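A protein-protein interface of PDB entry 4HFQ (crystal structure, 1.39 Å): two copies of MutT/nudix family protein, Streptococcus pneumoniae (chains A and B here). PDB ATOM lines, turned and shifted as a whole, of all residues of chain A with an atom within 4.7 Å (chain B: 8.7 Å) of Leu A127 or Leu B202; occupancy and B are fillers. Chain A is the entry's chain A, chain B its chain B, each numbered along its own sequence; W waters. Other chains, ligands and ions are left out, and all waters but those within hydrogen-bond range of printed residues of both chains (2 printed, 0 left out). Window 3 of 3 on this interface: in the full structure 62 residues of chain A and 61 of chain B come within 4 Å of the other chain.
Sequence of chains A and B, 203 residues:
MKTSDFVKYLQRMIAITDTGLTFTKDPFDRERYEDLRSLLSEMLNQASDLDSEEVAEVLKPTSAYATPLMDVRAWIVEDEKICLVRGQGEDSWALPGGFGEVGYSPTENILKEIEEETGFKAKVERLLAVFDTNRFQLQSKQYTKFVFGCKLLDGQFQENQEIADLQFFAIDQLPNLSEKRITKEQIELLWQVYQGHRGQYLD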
ATOM      1  N   THR A 107       7.845   0.147  -7.057  1.00  0.00           N
ATOM      2  CA  THR A 107       7.751  -1.274  -7.398  1.00  0.00           C
ATOM      3  C   THR A 107       6.839  -1.494  -8.605  1.00  0.00           C
ATOM      4  O   THR A 107       7.114  -2.352  -9.440  1.00  0.00           O
ATOM      5  CB  THR A 107       7.337  -2.163  -6.214  1.00  0.00           C
ATOM      6  OG1 THR A 107       5.998  -1.848  -5.804  1.00  0.00           O
ATOM      7  CG2 THR A 107       8.320  -2.032  -5.041  1.00  0.00           C
ATOM      8  N   ARG A 126      13.047  -7.648  -2.987  1.00  0.00           N
ATOM      9  CA  ARG A 126      13.717  -6.688  -2.098  1.00  0.00           C
ATOM     10  C   ARG A 126      14.378  -5.612  -2.934  1.00  0.00           C
ATOM     11  O   ARG A 126      14.534  -5.759  -4.144  1.00  0.00           O
ATOM     12  CB  ARG A 126      14.753  -7.384  -1.194  1.00  0.00           C
ATOM     13  CG  ARG A 126      15.914  -8.000  -1.960  1.00  0.00           C
ATOM     14  CD  ARG A 126      16.914  -8.714  -1.051  1.00  0.00           C
ATOM     15  NE  ARG A 126      17.725  -7.769  -0.283  1.00  0.00           N
ATOM     16  CZ  ARG A 126      18.997  -7.973   0.067  1.00  0.00           C
ATOM     17  NH1 ARG A 126      19.635  -9.073  -0.314  1.00  0.00           N
ATOM     18  NH2 ARG A 126      19.631  -7.055   0.776  1.00  0.00           N
ATOM     19  N   LEU A 127      14.761  -4.528  -2.276  1.00  0.00           N
ATOM     20  CA  LEU A 127      15.590  -3.507  -2.900  1.00  0.00           C
ATOM     21  C   LEU A 127      17.046  -3.847  -2.590  1.00  0.00           C
ATOM     22  O   LEU A 127      17.413  -3.973  -1.408  1.00  0.00           O
ATOM     23  CB  LEU A 127      15.222  -2.122  -2.360  1.00  0.00           C
ATOM     24  CG  LEU A 127      16.043  -0.920  -2.840  1.00  0.00           C
ATOM     25  CD1 LEU A 127      15.902  -0.739  -4.339  1.00  0.00           C
ATOM     26  CD2 LEU A 127      15.565   0.320  -2.098  1.00  0.00           C
ATOM     27  N   LEU A 128      17.875  -4.020  -3.624  1.00  0.00           N
ATOM     28  CA  LEU A 128      19.287  -4.371  -3.423  1.00  0.00           C
ATOM     29  C   LEU A 128      20.187  -3.147  -3.304  1.00  0.00           C
ATOM     30  O   LEU A 128      21.189  -3.175  -2.582  1.00  0.00           O
ATOM     31  CB  LEU A 128      19.804  -5.278  -4.540  1.00  0.00           C
ATOM     32  CG  LEU A 128      19.074  -6.617  -4.689  1.00  0.00           C
ATOM     33  CD1 LEU A 128      19.485  -7.231  -6.008  1.00  0.00           C
ATOM     34  CD2 LEU A 128      19.389  -7.576  -3.552  1.00  0.00           C
ATOM     35  N   ALA A 129      19.872  -2.081  -4.050  1.00  0.00           N
ATOM     36  CA  ALA A 129      20.757  -0.922  -4.108  1.00  0.00           C
ATOM     37  C   ALA A 129      19.996   0.284  -4.540  1.00  0.00           C
ATOM     38  O   ALA A 129      19.039   0.183  -5.328  1.00  0.00           O
ATOM     39  CB  ALA A 129      21.891  -1.154  -5.101  1.00  0.00           C
ATOM     40  N   VAL A 130      20.473   1.445  -4.079  1.00  0.00           N
ATOM     41  CA  VAL A 130      20.117   2.717  -4.724  1.00  0.00           C
ATOM     42  C   VAL A 130      21.437   3.382  -5.109  1.00  0.00           C
ATOM     43  O   VAL A 130      22.186   3.834  -4.239  1.00  0.00           O
ATOM     44  CB  VAL A 130      19.281   3.656  -3.822  1.00  0.00           C
ATOM     45  CG1 VAL A 130      18.880   4.901  -4.607  1.00  0.00           C
ATOM     46  CG2 VAL A 130      18.034   2.952  -3.312  1.00  0.00           C
ATOM     47  N   PHE A 146      17.385   2.689  -8.658  1.00  0.00           N
ATOM     48  CA  PHE A 146      16.894   1.623  -7.760  1.00  0.00           C
ATOM     49  C   PHE A 146      17.116   0.299  -8.474  1.00  0.00           C
ATOM     50  O   PHE A 146      16.710   0.144  -9.626  1.00  0.00           O
ATOM     51  CB  PHE A 146      15.386   1.760  -7.553  1.00  0.00           C
ATOM     52  CG  PHE A 146      14.960   2.963  -6.768  1.00  0.00           C
ATOM     53  CD1 PHE A 146      14.789   4.186  -7.390  1.00  0.00           C
ATOM     54  CD2 PHE A 146      14.688   2.862  -5.403  1.00  0.00           C
ATOM     55  CE1 PHE A 146      14.364   5.302  -6.681  1.00  0.00           C
ATOM     56  CE2 PHE A 146      14.270   3.975  -4.680  1.00  0.00           C
ATOM     57  CZ  PHE A 146      14.135   5.199  -5.313  1.00  0.00           C
ATOM     58  N   VAL A 147      17.735  -0.655  -7.793  1.00  0.00           N
ATOM     59  CA  VAL A 147      17.857  -2.007  -8.344  1.00  0.00           C
ATOM     60  C   VAL A 147      17.132  -2.963  -7.411  1.00  0.00           C
ATOM     61  O   VAL A 147      17.547  -3.154  -6.259  1.00  0.00           O
ATOM     62  CB  VAL A 147      19.318  -2.444  -8.522  1.00  0.00           C
ATOM     63  CG1 VAL A 147      19.339  -3.787  -9.229  1.00  0.00           C
ATOM     64  CG2 VAL A 147      20.104  -1.396  -9.311  1.00  0.00           C
ATOM     65  N   PHE A 148      16.031  -3.525  -7.915  1.00  0.00           N
ATOM     66  CA  PHE A 148      15.180  -4.426  -7.161  1.00  0.00           C
ATOM     67  C   PHE A 148      15.502  -5.869  -7.498  1.00  0.00           C
ATOM     68  O   PHE A 148      15.594  -6.233  -8.670  1.00  0.00           O
ATOM     69  CB  PHE A 148      13.711  -4.188  -7.514  1.00  0.00           C
ATOM     70  CG  PHE A 148      13.192  -2.833  -7.101  1.00  0.00           C
ATOM     71  CD1 PHE A 148      12.734  -2.618  -5.807  1.00  0.00           C
ATOM     72  CD2 PHE A 148      13.137  -1.791  -8.020  1.00  0.00           C
ATOM     73  CE1 PHE A 148      12.230  -1.372  -5.428  1.00  0.00           C
ATOM     74  CE2 PHE A 148      12.622  -0.551  -7.653  1.00  0.00           C
ATOM     75  CZ  PHE A 148      12.178  -0.347  -6.360  1.00  0.00           C
ATOM     76  N   GLN A 200      22.289  -3.965   1.921  1.00  0.00           N
ATOM     77  CA  GLN A 200      21.828  -3.043   0.897  1.00  0.00           C
ATOM     78  C   GLN A 200      22.845  -1.936   0.594  1.00  0.00           C
ATOM     79  O   GLN A 200      23.380  -1.308   1.513  1.00  0.00           O
ATOM     80  CB  GLN A 200      20.537  -2.414   1.402  1.00  0.00           C
ATOM     81  CG  GLN A 200      19.902  -1.493   0.377  1.00  0.00           C
ATOM     82  CD  GLN A 200      18.511  -1.126   0.801  1.00  0.00           C
ATOM     83  OE1 GLN A 200      17.530  -1.753   0.374  1.00  0.00           O
ATOM     84  NE2 GLN A 200      18.410  -0.136   1.676  1.00  0.00           N
ATOM     85  N   LEU B 127      18.211   2.913   5.227  1.00  0.00           N
ATOM     86  CA  LEU B 127      16.982   3.356   4.592  1.00  0.00           C
ATOM     87  C   LEU B 127      15.818   2.550   5.182  1.00  0.00           C
ATOM     88  O   LEU B 127      15.808   1.307   5.123  1.00  0.00           O
ATOM     89  CB  LEU B 127      17.100   3.135   3.081  1.00  0.00           C
ATOM     90  CG  LEU B 127      15.908   3.514   2.187  1.00  0.00           C
ATOM     91  CD1 LEU B 127      15.587   4.992   2.278  1.00  0.00           C
ATOM     92  CD2 LEU B 127      16.262   3.129   0.752  1.00  0.00           C
ATOM     93  N   LEU B 128      14.841   3.234   5.767  1.00  0.00           N
ATOM     94  CA  LEU B 128      13.703   2.550   6.382  1.00  0.00           C
ATOM     95  C   LEU B 128      12.537   2.323   5.423  1.00  0.00           C
ATOM     96  O   LEU B 128      11.845   1.315   5.530  1.00  0.00           O
ATOM     97  CB  LEU B 128      13.186   3.351   7.579  1.00  0.00           C
ATOM     98  CG  LEU B 128      14.162   3.481   8.759  1.00  0.00           C
ATOM     99  CD1 LEU B 128      13.648   4.511   9.751  1.00  0.00           C
ATOM    100  CD2 LEU B 128      14.369   2.141   9.469  1.00  0.00           C
ATOM    101  N   ALA B 129      12.322   3.241   4.485  1.00  0.00           N
ATOM    102  CA  ALA B 129      11.148   3.174   3.620  1.00  0.00           C
ATOM    103  C   ALA B 129      11.400   3.975   2.369  1.00  0.00           C
ATOM    104  O   ALA B 129      12.108   4.989   2.391  1.00  0.00           O
ATOM    105  CB  ALA B 129       9.905   3.721   4.324  1.00  0.00           C
ATOM    106  N   VAL B 130      10.762   3.537   1.291  1.00  0.00           N
ATOM    107  CA  VAL B 130      10.591   4.353   0.081  1.00  0.00           C
ATOM    108  C   VAL B 130       9.088   4.430  -0.155  1.00  0.00           C
ATOM    109  O   VAL B 130       8.466   3.454  -0.601  1.00  0.00           O
ATOM    110  CB  VAL B 130      11.333   3.781  -1.148  1.00  0.00           C
ATOM    111  CG1 VAL B 130      11.182   4.730  -2.336  1.00  0.00           C
ATOM    112  CG2 VAL B 130      12.808   3.567  -0.845  1.00  0.00           C
ATOM    113  N   PHE B 131       8.500   5.572   0.194  1.00  0.00           N
ATOM    114  CA  PHE B 131       7.068   5.771   0.049  1.00  0.00           C
ATOM    115  C   PHE B 131       6.696   6.437  -1.279  1.00  0.00           C
ATOM    116  O   PHE B 131       7.454   7.252  -1.824  1.00  0.00           O
ATOM    117  CB  PHE B 131       6.539   6.675   1.173  1.00  0.00           C
ATOM    118  CG  PHE B 131       6.511   6.052   2.552  1.00  0.00           C
ATOM    119  CD1 PHE B 131       5.706   4.952   2.829  1.00  0.00           C
ATOM    120  CD2 PHE B 131       7.249   6.609   3.572  1.00  0.00           C
ATOM    121  CE1 PHE B 131       5.663   4.416   4.119  1.00  0.00           C
ATOM    122  CE2 PHE B 131       7.214   6.081   4.860  1.00  0.00           C
ATOM    123  CZ  PHE B 131       6.415   4.976   5.129  1.00  0.00           C
ATOM    124  N   ASP B 132       5.533   6.067  -1.788  1.00  0.00           N
ATOM    125  CA  ASP B 132       4.921   6.786  -2.904  1.00  0.00           C
ATOM    126  C   ASP B 132       3.892   7.750  -2.335  1.00  0.00           C
ATOM    127  O   ASP B 132       2.938   7.334  -1.666  1.00  0.00           O
ATOM    128  CB  ASP B 132       4.269   5.781  -3.855  1.00  0.00           C
ATOM    129  CG  ASP B 132       3.631   6.431  -5.086  1.00  0.00           C
ATOM    130  OD1 ASP B 132       3.740   7.665  -5.271  1.00  0.00           O
ATOM    131  OD2 ASP B 132       3.011   5.658  -5.853  1.00  0.00           O
ATOM    132  N   ARG B 135       0.171   7.061  -2.742  1.00  0.00           N
ATOM    133  CA  ARG B 135      -0.543   6.141  -1.841  1.00  0.00           C
ATOM    134  C   ARG B 135      -0.957   6.811  -0.532  1.00  0.00           C
ATOM    135  O   ARG B 135      -2.059   6.579  -0.041  1.00  0.00           O
ATOM    136  CB  ARG B 135       0.293   4.899  -1.559  1.00  0.00           C
ATOM    137  CG  ARG B 135      -0.316   4.090  -0.430  1.00  0.00           C
ATOM    138  CD  ARG B 135       0.143   2.660  -0.372  1.00  0.00           C
ATOM    139  NE  ARG B 135      -0.586   2.029   0.725  1.00  0.00           N
ATOM    140  CZ  ARG B 135      -0.675   0.721   0.951  1.00  0.00           C
ATOM    141  NH1 ARG B 135      -0.064  -0.146   0.159  1.00  0.00           N
ATOM    142  NH2 ARG B 135      -1.379   0.290   1.997  1.00  0.00           N
ATOM    143  N   PHE B 136      -0.077   7.627   0.041  1.00  0.00           N
ATOM    144  CA  PHE B 136      -0.268   8.100   1.404  1.00  0.00           C
ATOM    145  C   PHE B 136      -0.742   9.531   1.543  1.00  0.00           C
ATOM    146  O   PHE B 136      -1.331   9.905   2.564  1.00  0.00           O
ATOM    147  CB  PHE B 136       1.018   7.902   2.216  1.00  0.00           C
ATOM    148  CG  PHE B 136       1.311   6.467   2.546  1.00  0.00           C
ATOM    149  CD1 PHE B 136       0.716   5.870   3.661  1.00  0.00           C
ATOM    150  CD2 PHE B 136       2.129   5.695   1.736  1.00  0.00           C
ATOM    151  CE1 PHE B 136       0.958   4.541   3.963  1.00  0.00           C
ATOM    152  CE2 PHE B 136       2.347   4.361   2.034  1.00  0.00           C
ATOM    153  CZ  PHE B 136       1.783   3.786   3.156  1.00  0.00           C
ATOM    154  N   THR B 144       8.783  10.338  -4.789  1.00  0.00           N
ATOM    155  CA  THR B 144       9.401   9.168  -4.190  1.00  0.00           C
ATOM    156  C   THR B 144      10.061   9.650  -2.926  1.00  0.00           C
ATOM    157  O   THR B 144      11.005  10.444  -2.977  1.00  0.00           O
ATOM    158  CB  THR B 144      10.443   8.596  -5.143  1.00  0.00           C
ATOM    159  OG1 THR B 144       9.770   8.209  -6.343  1.00  0.00           O
ATOM    160  CG2 THR B 144      11.164   7.420  -4.544  1.00  0.00           C
ATOM    161  N   LYS B 145       9.524   9.197  -1.800  1.00  0.00           N
ATOM    162  CA  LYS B 145       9.891   9.727  -0.484  1.00  0.00           C
ATOM    163  C   LYS B 145      10.798   8.708   0.228  1.00  0.00           C
ATOM    164  O   LYS B 145      10.321   7.676   0.754  1.00  0.00           O
ATOM    165  CB  LYS B 145       8.609  10.023   0.312  1.00  0.00           C
ATOM    166  CG  LYS B 145       8.841  10.546   1.735  1.00  0.00           C
ATOM    167  CD  LYS B 145       7.516  10.822   2.469  1.00  0.00           C
ATOM    168  CE  LYS B 145       6.682  11.921   1.804  1.00  0.00           C
ATOM    169  NZ  LYS B 145       7.291  13.275   2.005  1.00  0.00           N
ATOM    170  N   PHE B 146      12.095   8.996   0.245  1.00  0.00           N
ATOM    171  CA  PHE B 146      13.071   8.172   0.949  1.00  0.00           C
ATOM    172  C   PHE B 146      13.034   8.551   2.420  1.00  0.00           C
ATOM    173  O   PHE B 146      13.131   9.742   2.738  1.00  0.00           O
ATOM    174  CB  PHE B 146      14.487   8.526   0.479  1.00  0.00           C
ATOM    175  CG  PHE B 146      14.841   8.153  -0.934  1.00  0.00           C
ATOM    176  CD1 PHE B 146      14.378   8.877  -2.041  1.00  0.00           C
ATOM    177  CD2 PHE B 146      15.768   7.131  -1.146  1.00  0.00           C
ATOM    178  CE1 PHE B 146      14.818   8.538  -3.342  1.00  0.00           C
ATOM    179  CE2 PHE B 146      16.198   6.799  -2.423  1.00  0.00           C
ATOM    180  CZ  PHE B 146      15.719   7.490  -3.514  1.00  0.00           C
ATOM    181  N   LEU B 189       4.134   2.950  10.499  1.00  0.00           N
ATOM    182  CA  LEU B 189       4.882   1.971   9.722  1.00  0.00           C
ATOM    183  C   LEU B 189       6.375   2.102   9.973  1.00  0.00           C
ATOM    184  O   LEU B 189       7.065   1.100  10.196  1.00  0.00           O
ATOM    185  CB  LEU B 189       4.587   2.107   8.217  1.00  0.00           C
ATOM    186  CG  LEU B 189       3.235   1.566   7.731  1.00  0.00           C
ATOM    187  CD1 LEU B 189       2.864   2.105   6.347  1.00  0.00           C
ATOM    188  CD2 LEU B 189       3.258   0.046   7.676  1.00  0.00           C
ATOM    189  N   VAL B 193       9.244  -0.636  11.267  1.00  0.00           N
ATOM    190  CA  VAL B 193      10.482  -0.962  10.573  1.00  0.00           C
ATOM    191  C   VAL B 193      11.688  -0.692  11.470  1.00  0.00           C
ATOM    192  O   VAL B 193      12.607  -1.524  11.574  1.00  0.00           O
ATOM    193  CB  VAL B 193      10.630  -0.161   9.241  1.00  0.00           C
ATOM    194  CG1 VAL B 193      11.909  -0.545   8.508  1.00  0.00           C
ATOM    195  CG2 VAL B 193       9.439  -0.381   8.316  1.00  0.00           C
ATOM    196  N   ARG B 198       9.115  -5.315  11.031  1.00  0.00           N
ATOM    197  CA  ARG B 198       8.822  -5.617   9.620  1.00  0.00           C
ATOM    198  C   ARG B 198      10.012  -5.118   8.827  1.00  0.00           C
ATOM    199  O   ARG B 198      10.847  -4.377   9.354  1.00  0.00           O
ATOM    200  CB  ARG B 198       7.519  -5.006   9.102  1.00  0.00           C
ATOM    201  CG  ARG B 198       7.458  -3.501   9.238  1.00  0.00           C
ATOM    202  CD  ARG B 198       6.070  -2.934   8.843  1.00  0.00           C
ATOM    203  NE  ARG B 198       5.695  -3.272   7.467  1.00  0.00           N
ATOM    204  CZ  ARG B 198       4.457  -3.540   7.027  1.00  0.00           C
ATOM    205  NH1 ARG B 198       3.391  -3.519   7.825  1.00  0.00           N
ATOM    206  NH2 ARG B 198       4.288  -3.847   5.760  1.00  0.00           N
ATOM    207  N   GLY B 199      10.115  -5.563   7.590  1.00  0.00           N
ATOM    208  CA  GLY B 199      11.253  -5.222   6.752  1.00  0.00           C
ATOM    209  C   GLY B 199      11.131  -3.832   6.164  1.00  0.00           C
ATOM    210  O   GLY B 199      10.097  -3.160   6.308  1.00  0.00           O
ATOM    211  N   GLN B 200      12.182  -3.425   5.464  1.00  0.00           N
ATOM    212  CA  GLN B 200      12.163  -2.146   4.765  1.00  0.00           C
ATOM    213  C   GLN B 200      10.863  -2.010   3.988  1.00  0.00           C
ATOM    214  O   GLN B 200      10.474  -2.914   3.261  1.00  0.00           O
ATOM    215  CB  GLN B 200      13.326  -2.116   3.804  1.00  0.00           C
ATOM    216  CG  GLN B 200      13.437  -0.819   3.026  1.00  0.00           C
ATOM    217  CD  GLN B 200      14.695  -0.810   2.203  1.00  0.00           C
ATOM    218  OE1 GLN B 200      14.796  -1.498   1.194  1.00  0.00           O
ATOM    219  NE2 GLN B 200      15.691  -0.083   2.669  1.00  0.00           N
ATOM    220  N   TYR B 201      10.212  -0.862   4.114  1.00  0.00           N
ATOM    221  CA  TYR B 201       8.923  -0.649   3.464  1.00  0.00           C
ATOM    222  C   TYR B 201       9.101  -0.066   2.060  1.00  0.00           C
ATOM    223  O   TYR B 201       9.751   0.973   1.907  1.00  0.00           O
ATOM    224  CB  TYR B 201       8.070   0.298   4.315  1.00  0.00           C
ATOM    225  CG  TYR B 201       6.703   0.471   3.708  1.00  0.00           C
ATOM    226  CD1 TYR B 201       6.504   1.388   2.682  1.00  0.00           C
ATOM    227  CD2 TYR B 201       5.627  -0.324   4.102  1.00  0.00           C
ATOM    228  CE1 TYR B 201       5.280   1.520   2.058  1.00  0.00           C
ATOM    229  CE2 TYR B 201       4.388  -0.200   3.488  1.00  0.00           C
ATOM    230  CZ  TYR B 201       4.228   0.730   2.470  1.00  0.00           C
ATOM    231  OH  TYR B 201       3.007   0.848   1.859  1.00  0.00           O
ATOM    232  N   LEU B 202       8.515  -0.704   1.057  1.00  0.00           N
ATOM    233  CA  LEU B 202       8.577  -0.213  -0.322  1.00  0.00           C
ATOM    234  C   LEU B 202       7.192  -0.150  -0.924  1.00  0.00           C
ATOM    235  O   LEU B 202       6.501  -1.163  -0.966  1.00  0.00           O
ATOM    236  CB  LEU B 202       9.392  -1.171  -1.184  1.00  0.00           C
ATOM    237  CG  LEU B 202      10.821  -1.496  -0.735  1.00  0.00           C
ATOM    238  CD1 LEU B 202      11.427  -2.641  -1.543  1.00  0.00           C
ATOM    239  CD2 LEU B 202      11.716  -0.267  -0.790  1.00  0.00           C
ATOM    240  N   ASP B 203       6.771   1.014  -1.404  1.00  0.00           N
ATOM    241  CA  ASP B 203       5.556   1.075  -2.247  1.00  0.00           C
ATOM    242  C   ASP B 203       5.848   0.607  -3.669  1.00  0.00           C
ATOM    243  O   ASP B 203       6.938   0.797  -4.188  1.00  0.00           O
ATOM    244  CB  ASP B 203       4.972   2.496  -2.266  1.00  0.00           C
ATOM    245  CG  ASP B 203       4.182   2.818  -1.021  1.00  0.00           C
ATOM    246  OD1 ASP B 203       3.371   1.964  -0.570  1.00  0.00           O
ATOM    247  OD2 ASP B 203       4.337   3.924  -0.481  1.00  0.00           O
HETATM  248  O   HOH W   1      14.179  -4.116   0.545  1.00  0.00           O
HETATM  249  O   HOH W   2      19.350   0.436   4.212  1.00  0.00           O
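CB of Leu A127 touches OE1 of Gln B200, at 3.6 Å.
Leu A127 touches Leu B202.
CE2 of Phe B146 touches CG1 of Val A130 (3.9 Å).
Phe A146 touches Val B130 (CE2 to CG1, 3.9 Å).
Phe A146 touches Thr B144.
CZ of Phe A146 touches CZ of Phe B146 (3.3 Å).
Gln A200 touches Leu B127.
Of chain A, only Leu A127 (3.9 Å) comes within 4 Å of Leu B202.
Of the printed residues of chain B, Phe A146 touches Val B130, Thr B144 and Phe B146.
Of the printed residues of chain A, Gln B200 touches Leu A127 and Gln A200.
Of the printed residues of chain A, Leu B127 touches Gln A200 (3.8 Å).
Of the printed residues of chain A, Val B130 touches Phe A146 (3.9 Å).
The nearest residue of chain B that does not touch Leu A127 is Leu B127 (4.1 Å).
The nearest residue of chain A that does not touch Leu B202 is Thr A107 (4.1 Å).
Water W2 bridges the side-chain amide nitrogen (NE2) of Gln A200 and the backbone NH (N) of Leu B127.
Water W1 lies within hydrogen-bond range of OE1 of Gln B200 and N of Leu A127.
N of Thr A107 is in hydrogen-bond range of O of Asp B203 (3.1 Å).
The side-chain amide oxygen (OE1) of Gln B200 lies close to the side-chain amide oxygen (OE1) of Gln A200 (2.9 Å).
O of Leu A127 sits close to OE1 of Gln A200 (2.8 Å).
NE2 of Gln B200 is in hydrogen-bond range of O of Leu B127 (2.8 Å).
O of Tyr B201 sits at hydrogen-bond distance from N of Val B130 (2.8 Å).
O of Val B130 lies within hydrogen-bond range of N of Asp B203, at 3.1 Å.
The side-chain carboxylate (OD2) of Asp B203 lies within hydrogen-bond range of the backbone NH (N) of Asp B132 (2.8 Å).
OH of Tyr B201 sits at hydrogen-bond distance from OD1 of Asp B203, 2.7 Å away.
Leu A127 touches Gln B200, and with the chains exchanged Gln A200 touches Leu B127.
Val A130 touches Phe B146, and with the chains exchanged Phe A146 touches Val B130.
Phe A146 touches its own counterpart, Phe B146.
Gln B200 touches its own counterpart, Gln A200.
Of the 10 printed residues of chain A, 5 touch a printed residue of chain B.
Printed residues of chain A that touch a printed residue of chain B: Thr A107, Leu A127, Val A130, Phe A146 and Gln A200.
Hydrophobic or aromatic side chains of chain A that line the printed part of chain B: Leu A127, Val A130 and Phe A146.
Of the 19 printed residues of chain B, 7 touch a printed residue of chain A.
Hydrophobic or aromatic side chains of chain B within 4 Å of the printed part of chain A: Leu B127, Val B130, Phe B146 and Leu B202.
Among the printed residues, 9 pairs touch across the chains.
Among the printed residues, no Asp or Glu carboxylate lies within 4 Å of a Lys or Arg side-chain nitrogen of the other chain.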
